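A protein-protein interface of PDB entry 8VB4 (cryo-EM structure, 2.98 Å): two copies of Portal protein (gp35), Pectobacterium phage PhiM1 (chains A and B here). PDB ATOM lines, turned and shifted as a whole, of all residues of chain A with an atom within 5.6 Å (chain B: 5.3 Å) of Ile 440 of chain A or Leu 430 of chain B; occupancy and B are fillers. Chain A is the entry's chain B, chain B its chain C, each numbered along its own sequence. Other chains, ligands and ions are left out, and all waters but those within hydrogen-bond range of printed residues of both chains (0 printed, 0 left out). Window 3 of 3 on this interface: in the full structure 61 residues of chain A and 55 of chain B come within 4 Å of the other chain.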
ATOM      1  N   SER A 436      33.056  22.437  26.151  1.00  0.00           N
ATOM      2  CA  SER A 436      31.926  21.945  25.371  1.00  0.00           C
ATOM      3  C   SER A 436      30.584  22.413  25.922  1.00  0.00           C
ATOM      4  O   SER A 436      29.683  22.747  25.138  1.00  0.00           O
ATOM      5  CB  SER A 436      31.953  20.418  25.317  1.00  0.00           C
ATOM      6  OG  SER A 436      33.119  19.957  24.657  1.00  0.00           O
ATOM      7  N   LEU A 437      30.431  22.443  27.244  1.00  0.00           N
ATOM      8  CA  LEU A 437      29.208  22.913  27.873  1.00  0.00           C
ATOM      9  C   LEU A 437      28.940  24.383  27.592  1.00  0.00           C
ATOM     10  O   LEU A 437      27.782  24.810  27.658  1.00  0.00           O
ATOM     11  CB  LEU A 437      29.296  22.685  29.388  1.00  0.00           C
ATOM     12  CG  LEU A 437      28.991  21.299  29.978  1.00  0.00           C
ATOM     13  CD1 LEU A 437      28.764  21.427  31.474  1.00  0.00           C
ATOM     14  CD2 LEU A 437      27.797  20.608  29.340  1.00  0.00           C
ATOM     15  N   SER A 438      29.977  25.165  27.283  1.00  0.00           N
ATOM     16  CA  SER A 438      29.796  26.564  26.926  1.00  0.00           C
ATOM     17  C   SER A 438      29.368  26.743  25.477  1.00  0.00           C
ATOM     18  O   SER A 438      29.014  27.858  25.084  1.00  0.00           O
ATOM     19  CB  SER A 438      31.090  27.343  27.166  1.00  0.00           C
ATOM     20  OG  SER A 438      32.111  26.905  26.289  1.00  0.00           O
ATOM     21  N   VAL A 439      29.411  25.678  24.679  1.00  0.00           N
ATOM     22  CA  VAL A 439      28.956  25.727  23.302  1.00  0.00           C
ATOM     23  C   VAL A 439      27.609  25.037  23.113  1.00  0.00           C
ATOM     24  O   VAL A 439      26.845  25.437  22.229  1.00  0.00           O
ATOM     25  CB  VAL A 439      30.016  25.114  22.363  1.00  0.00           C
ATOM     26  CG1 VAL A 439      29.450  24.930  20.961  1.00  0.00           C
ATOM     27  CG2 VAL A 439      31.263  25.979  22.332  1.00  0.00           C
ATOM     28  N   ILE A 440      27.295  24.022  23.916  1.00  0.00           N
ATOM     29  CA  ILE A 440      26.052  23.277  23.719  1.00  0.00           C
ATOM     30  C   ILE A 440      24.880  23.924  24.452  1.00  0.00           C
ATOM     31  O   ILE A 440      23.757  23.928  23.947  1.00  0.00           O
ATOM     32  CB  ILE A 440      26.238  21.807  24.145  1.00  0.00           C
ATOM     33  CG1 ILE A 440      27.455  21.186  23.450  1.00  0.00           C
ATOM     34  CG2 ILE A 440      24.993  20.999  23.816  1.00  0.00           C
ATOM     35  CD1 ILE A 440      27.892  19.866  24.047  1.00  0.00           C
ATOM     36  N   LEU A 441      25.104  24.485  25.640  1.00  0.00           N
ATOM     37  CA  LEU A 441      23.998  25.013  26.438  1.00  0.00           C
ATOM     38  C   LEU A 441      23.465  26.338  25.903  1.00  0.00           C
ATOM     39  O   LEU A 441      22.256  26.582  25.988  1.00  0.00           O
ATOM     40  CB  LEU A 441      24.403  25.177  27.905  1.00  0.00           C
ATOM     41  CG  LEU A 441      24.424  23.881  28.721  1.00  0.00           C
ATOM     42  CD1 LEU A 441      25.580  22.981  28.340  1.00  0.00           C
ATOM     43  CD2 LEU A 441      24.442  24.175  30.216  1.00  0.00           C
ATOM     44  N   PRO A 442      24.309  27.230  25.377  1.00  0.00           N
ATOM     45  CA  PRO A 442      23.751  28.456  24.779  1.00  0.00           C
ATOM     46  C   PRO A 442      22.692  28.158  23.734  1.00  0.00           C
ATOM     47  O   PRO A 442      21.683  28.870  23.649  1.00  0.00           O
ATOM     48  CB  PRO A 442      24.990  29.135  24.186  1.00  0.00           C
ATOM     49  CG  PRO A 442      26.081  28.714  25.089  1.00  0.00           C
ATOM     50  CD  PRO A 442      25.782  27.273  25.404  1.00  0.00           C
ATOM     51  N   VAL A 443      22.898  27.114  22.929  1.00  0.00           N
ATOM     52  CA  VAL A 443      21.820  26.577  22.111  1.00  0.00           C
ATOM     53  C   VAL A 443      20.955  25.672  22.980  1.00  0.00           C
ATOM     54  O   VAL A 443      21.381  25.200  24.042  1.00  0.00           O
ATOM     55  CB  VAL A 443      22.387  25.818  20.897  1.00  0.00           C
ATOM     56  CG1 VAL A 443      21.265  25.287  20.021  1.00  0.00           C
ATOM     57  CG2 VAL A 443      23.318  26.715  20.094  1.00  0.00           C
ATOM     58  N   PHE A 444      19.725  25.427  22.532  1.00  0.00           N
ATOM     59  CA  PHE A 444      18.714  24.636  23.234  1.00  0.00           C
ATOM     60  C   PHE A 444      18.105  25.412  24.394  1.00  0.00           C
ATOM     61  O   PHE A 444      17.256  24.862  25.111  1.00  0.00           O
ATOM     62  CB  PHE A 444      19.256  23.308  23.773  1.00  0.00           C
ATOM     63  CG  PHE A 444      19.874  22.428  22.723  1.00  0.00           C
ATOM     64  CD1 PHE A 444      19.165  22.073  21.591  1.00  0.00           C
ATOM     65  CD2 PHE A 444      21.164  21.952  22.874  1.00  0.00           C
ATOM     66  CE1 PHE A 444      19.733  21.263  20.627  1.00  0.00           C
ATOM     67  CE2 PHE A 444      21.736  21.141  21.913  1.00  0.00           C
ATOM     68  CZ  PHE A 444      21.018  20.798  20.788  1.00  0.00           C
ATOM     69  N   ILE A 455      21.428  16.474  29.150  1.00  0.00           N
ATOM     70  CA  ILE A 455      22.640  16.854  28.433  1.00  0.00           C
ATOM     71  C   ILE A 455      23.822  16.916  29.390  1.00  0.00           C
ATOM     72  O   ILE A 455      24.923  16.451  29.069  1.00  0.00           O
ATOM     73  CB  ILE A 455      22.435  18.196  27.706  1.00  0.00           C
ATOM     74  CG1 ILE A 455      21.455  18.032  26.546  1.00  0.00           C
ATOM     75  CG2 ILE A 455      23.767  18.735  27.208  1.00  0.00           C
ATOM     76  CD1 ILE A 455      20.850  19.334  26.073  1.00  0.00           C
ATOM     77  N   MET A 458      24.890  13.392  30.346  1.00  0.00           N
ATOM     78  CA  MET A 458      25.554  12.716  29.241  1.00  0.00           C
ATOM     79  C   MET A 458      26.959  13.236  28.995  1.00  0.00           C
ATOM     80  O   MET A 458      27.889  12.436  28.855  1.00  0.00           O
ATOM     81  CB  MET A 458      24.735  12.870  27.955  1.00  0.00           C
ATOM     82  CG  MET A 458      25.322  12.149  26.751  1.00  0.00           C
ATOM     83  SD  MET A 458      24.317  12.338  25.270  1.00  0.00           S
ATOM     84  CE  MET A 458      24.633  14.055  24.875  1.00  0.00           C
ATOM     85  N   VAL A 459      27.136  14.557  28.954  1.00  0.00           N
ATOM     86  CA  VAL A 459      28.454  15.120  28.685  1.00  0.00           C
ATOM     87  C   VAL A 459      29.427  14.780  29.805  1.00  0.00           C
ATOM     88  O   VAL A 459      30.580  14.421  29.547  1.00  0.00           O
ATOM     89  CB  VAL A 459      28.347  16.640  28.470  1.00  0.00           C
ATOM     90  CG1 VAL A 459      29.731  17.253  28.325  1.00  0.00           C
ATOM     91  CG2 VAL A 459      27.502  16.944  27.244  1.00  0.00           C
ATOM     92  N   ASP B 426      30.654  10.356  21.764  1.00  0.00           N
ATOM     93  CA  ASP B 426      29.315  10.820  21.420  1.00  0.00           C
ATOM     94  C   ASP B 426      29.205  12.335  21.535  1.00  0.00           C
ATOM     95  O   ASP B 426      28.340  12.943  20.894  1.00  0.00           O
ATOM     96  CB  ASP B 426      28.275  10.149  22.316  1.00  0.00           C
ATOM     97  CG  ASP B 426      28.318   8.638  22.228  1.00  0.00           C
ATOM     98  OD1 ASP B 426      29.207   8.106  21.530  1.00  0.00           O
ATOM     99  OD2 ASP B 426      27.458   7.983  22.852  1.00  0.00           O
ATOM    100  N   VAL B 427      30.066  12.959  22.342  1.00  0.00           N
ATOM    101  CA  VAL B 427      30.015  14.406  22.509  1.00  0.00           C
ATOM    102  C   VAL B 427      30.376  15.115  21.209  1.00  0.00           C
ATOM    103  O   VAL B 427      29.915  16.236  20.954  1.00  0.00           O
ATOM    104  CB  VAL B 427      30.940  14.834  23.663  1.00  0.00           C
ATOM    105  CG1 VAL B 427      32.394  14.545  23.320  1.00  0.00           C
ATOM    106  CG2 VAL B 427      30.742  16.308  23.987  1.00  0.00           C
ATOM    107  N   ASN B 428      31.209  14.490  20.373  1.00  0.00           N
ATOM    108  CA  ASN B 428      31.561  15.101  19.096  1.00  0.00           C
ATOM    109  C   ASN B 428      30.346  15.208  18.186  1.00  0.00           C
ATOM    110  O   ASN B 428      30.187  16.198  17.462  1.00  0.00           O
ATOM    111  CB  ASN B 428      32.668  14.298  18.419  1.00  0.00           C
ATOM    112  CG  ASN B 428      33.902  14.169  19.282  1.00  0.00           C
ATOM    113  OD1 ASN B 428      34.126  13.138  19.916  1.00  0.00           O
ATOM    114  ND2 ASN B 428      34.715  15.216  19.305  1.00  0.00           N
ATOM    115  N   LYS B 429      29.481  14.197  18.201  1.00  0.00           N
ATOM    116  CA  LYS B 429      28.266  14.201  17.400  1.00  0.00           C
ATOM    117  C   LYS B 429      27.215  15.160  17.937  1.00  0.00           C
ATOM    118  O   LYS B 429      26.303  15.539  17.196  1.00  0.00           O
ATOM    119  CB  LYS B 429      27.683  12.788  17.326  1.00  0.00           C
ATOM    120  CG  LYS B 429      28.275  11.933  16.221  1.00  0.00           C
ATOM    121  CD  LYS B 429      27.382  10.747  15.907  1.00  0.00           C
ATOM    122  CE  LYS B 429      27.055   9.958  17.163  1.00  0.00           C
ATOM    123  NZ  LYS B 429      28.090   8.929  17.453  1.00  0.00           N
ATOM    124  N   LEU B 430      27.319  15.563  19.202  1.00  0.00           N
ATOM    125  CA  LEU B 430      26.447  16.572  19.787  1.00  0.00           C
ATOM    126  C   LEU B 430      26.942  17.986  19.526  1.00  0.00           C
ATOM    127  O   LEU B 430      26.134  18.894  19.302  1.00  0.00           O
ATOM    128  CB  LEU B 430      26.325  16.345  21.296  1.00  0.00           C
ATOM    129  CG  LEU B 430      25.256  17.143  22.042  1.00  0.00           C
ATOM    130  CD1 LEU B 430      23.867  16.810  21.532  1.00  0.00           C
ATOM    131  CD2 LEU B 430      25.353  16.880  23.534  1.00  0.00           C
ATOM    132  N   ILE B 431      28.259  18.187  19.541  1.00  0.00           N
ATOM    133  CA  ILE B 431      28.819  19.508  19.262  1.00  0.00           C
ATOM    134  C   ILE B 431      28.465  19.941  17.843  1.00  0.00           C
ATOM    135  O   ILE B 431      28.111  21.099  17.596  1.00  0.00           O
ATOM    136  CB  ILE B 431      30.340  19.505  19.484  1.00  0.00           C
ATOM    137  CG1 ILE B 431      30.656  19.383  20.975  1.00  0.00           C
ATOM    138  CG2 ILE B 431      30.959  20.770  18.910  1.00  0.00           C
ATOM    139  CD1 ILE B 431      32.098  19.034  21.270  1.00  0.00           C
ATOM    140  N   GLN B 432      28.573  19.016  16.888  1.00  0.00           N
ATOM    141  CA  GLN B 432      28.253  19.341  15.501  1.00  0.00           C
ATOM    142  C   GLN B 432      26.784  19.719  15.352  1.00  0.00           C
ATOM    143  O   GLN B 432      26.442  20.684  14.652  1.00  0.00           O
ATOM    144  CB  GLN B 432      28.598  18.156  14.601  1.00  0.00           C
ATOM    145  CG  GLN B 432      30.042  18.126  14.142  1.00  0.00           C
ATOM    146  CD  GLN B 432      30.371  16.878  13.350  1.00  0.00           C
ATOM    147  OE1 GLN B 432      29.500  16.050  13.085  1.00  0.00           O
ATOM    148  NE2 GLN B 432      31.634  16.734  12.970  1.00  0.00           N
ATOM    149  N   ALA B 433      25.897  18.958  15.994  1.00  0.00           N
ATOM    150  CA  ALA B 433      24.476  19.276  15.940  1.00  0.00           C
ATOM    151  C   ALA B 433      24.202  20.643  16.549  1.00  0.00           C
ATOM    152  O   ALA B 433      23.404  21.421  16.013  1.00  0.00           O
ATOM    153  CB  ALA B 433      23.669  18.198  16.659  1.00  0.00           C
ATOM    154  N   ALA B 434      24.853  20.952  17.672  1.00  0.00           N
ATOM    155  CA  ALA B 434      24.675  22.264  18.286  1.00  0.00           C
ATOM    156  C   ALA B 434      25.160  23.373  17.363  1.00  0.00           C
ATOM    157  O   ALA B 434      24.515  24.420  17.252  1.00  0.00           O
ATOM    158  CB  ALA B 434      25.413  22.319  19.622  1.00  0.00           C
ATOM    159  N   GLN B 435      26.297  23.163  16.698  1.00  0.00           N
ATOM    160  CA  GLN B 435      26.812  24.177  15.784  1.00  0.00           C
ATOM    161  C   GLN B 435      25.866  24.412  14.616  1.00  0.00           C
ATOM    162  O   GLN B 435      25.625  25.565  14.241  1.00  0.00           O
ATOM    163  CB  GLN B 435      28.193  23.769  15.271  1.00  0.00           C
ATOM    164  CG  GLN B 435      29.297  23.896  16.305  1.00  0.00           C
ATOM    165  CD  GLN B 435      30.638  23.423  15.785  1.00  0.00           C
ATOM    166  OE1 GLN B 435      30.711  22.685  14.804  1.00  0.00           O
ATOM    167  NE2 GLN B 435      31.711  23.844  16.444  1.00  0.00           N
ATOM    168  N   ILE B 465      21.604  10.411  17.007  1.00  0.00           N
ATOM    169  CA  ILE B 465      21.366  10.568  18.438  1.00  0.00           C
ATOM    170  C   ILE B 465      19.964  10.076  18.756  1.00  0.00           C
ATOM    171  O   ILE B 465      18.985  10.511  18.135  1.00  0.00           O
ATOM    172  CB  ILE B 465      21.547  12.034  18.875  1.00  0.00           C
ATOM    173  CG1 ILE B 465      22.985  12.494  18.633  1.00  0.00           C
ATOM    174  CG2 ILE B 465      21.183  12.199  20.341  1.00  0.00           C
ATOM    175  CD1 ILE B 465      23.126  13.991  18.474  1.00  0.00           C
ATOM    176  N   LEU B 470      17.114  12.748  25.504  1.00  0.00           N
ATOM    177  CA  LEU B 470      17.177  14.199  25.638  1.00  0.00           C
ATOM    178  C   LEU B 470      15.815  14.843  25.836  1.00  0.00           C
ATOM    179  O   LEU B 470      15.691  15.775  26.632  1.00  0.00           O
ATOM    180  CB  LEU B 470      17.842  14.815  24.398  1.00  0.00           C
ATOM    181  CG  LEU B 470      19.201  14.239  23.997  1.00  0.00           C
ATOM    182  CD1 LEU B 470      19.632  14.793  22.651  1.00  0.00           C
ATOM    183  CD2 LEU B 470      20.247  14.530  25.057  1.00  0.00           C
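Ile 440 of chain A touches one residue of chain B. Of chain A, only Ile 440 and Met 458 come within 4 Å of Leu 430 of chain B. Of the printed residues of chain A, Ile 431 of chain B touches Ser 436 (3.7 Å). Of the printed residues of chain A, Ala 434 of chain B touches Val 443. Of the printed residues of chain B, Ile 455 of chain A touches Leu 470. Phe 444 of chain A touches none of the printed residues of chain B. Lys 429 of chain B touches none of the printed residues of chain A. The nearest residue of chain B that does not touch Ile 440 of chain A is Ile 431 of chain B (4.2 Å).
No position is printed for both chains. Of the 5 pairs that touch across the chains among the printed residues, none has its exchanged pair printed and touching as well.
Among the printed residues, merely in contact across the chains: Ser 436 of chain A with Ile 431 of chain B, Ile 440 of chain A with Leu 430 of chain B, Val 443 of chain A with Ala 434 of chain B, Ile 455 of chain A with Leu 470 of chain B and Met 458 of chain A with Leu 430 of chain B.
Of the 12 printed residues of chain A, 5 touch a printed residue of chain B. Hydrophobic or aromatic side chains of chain A that line the printed part of chain B: Ile 440, Val 443, Ile 455 and Met 458. Hydrophobic or aromatic side chains of chain B that line the printed part of chain A: Leu 430, Ile 431 and Leu 470. Among the printed residues, no Asp or Glu carboxylate lies within 4 Å of a Lys or Arg side-chain nitrogen of the other chain.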
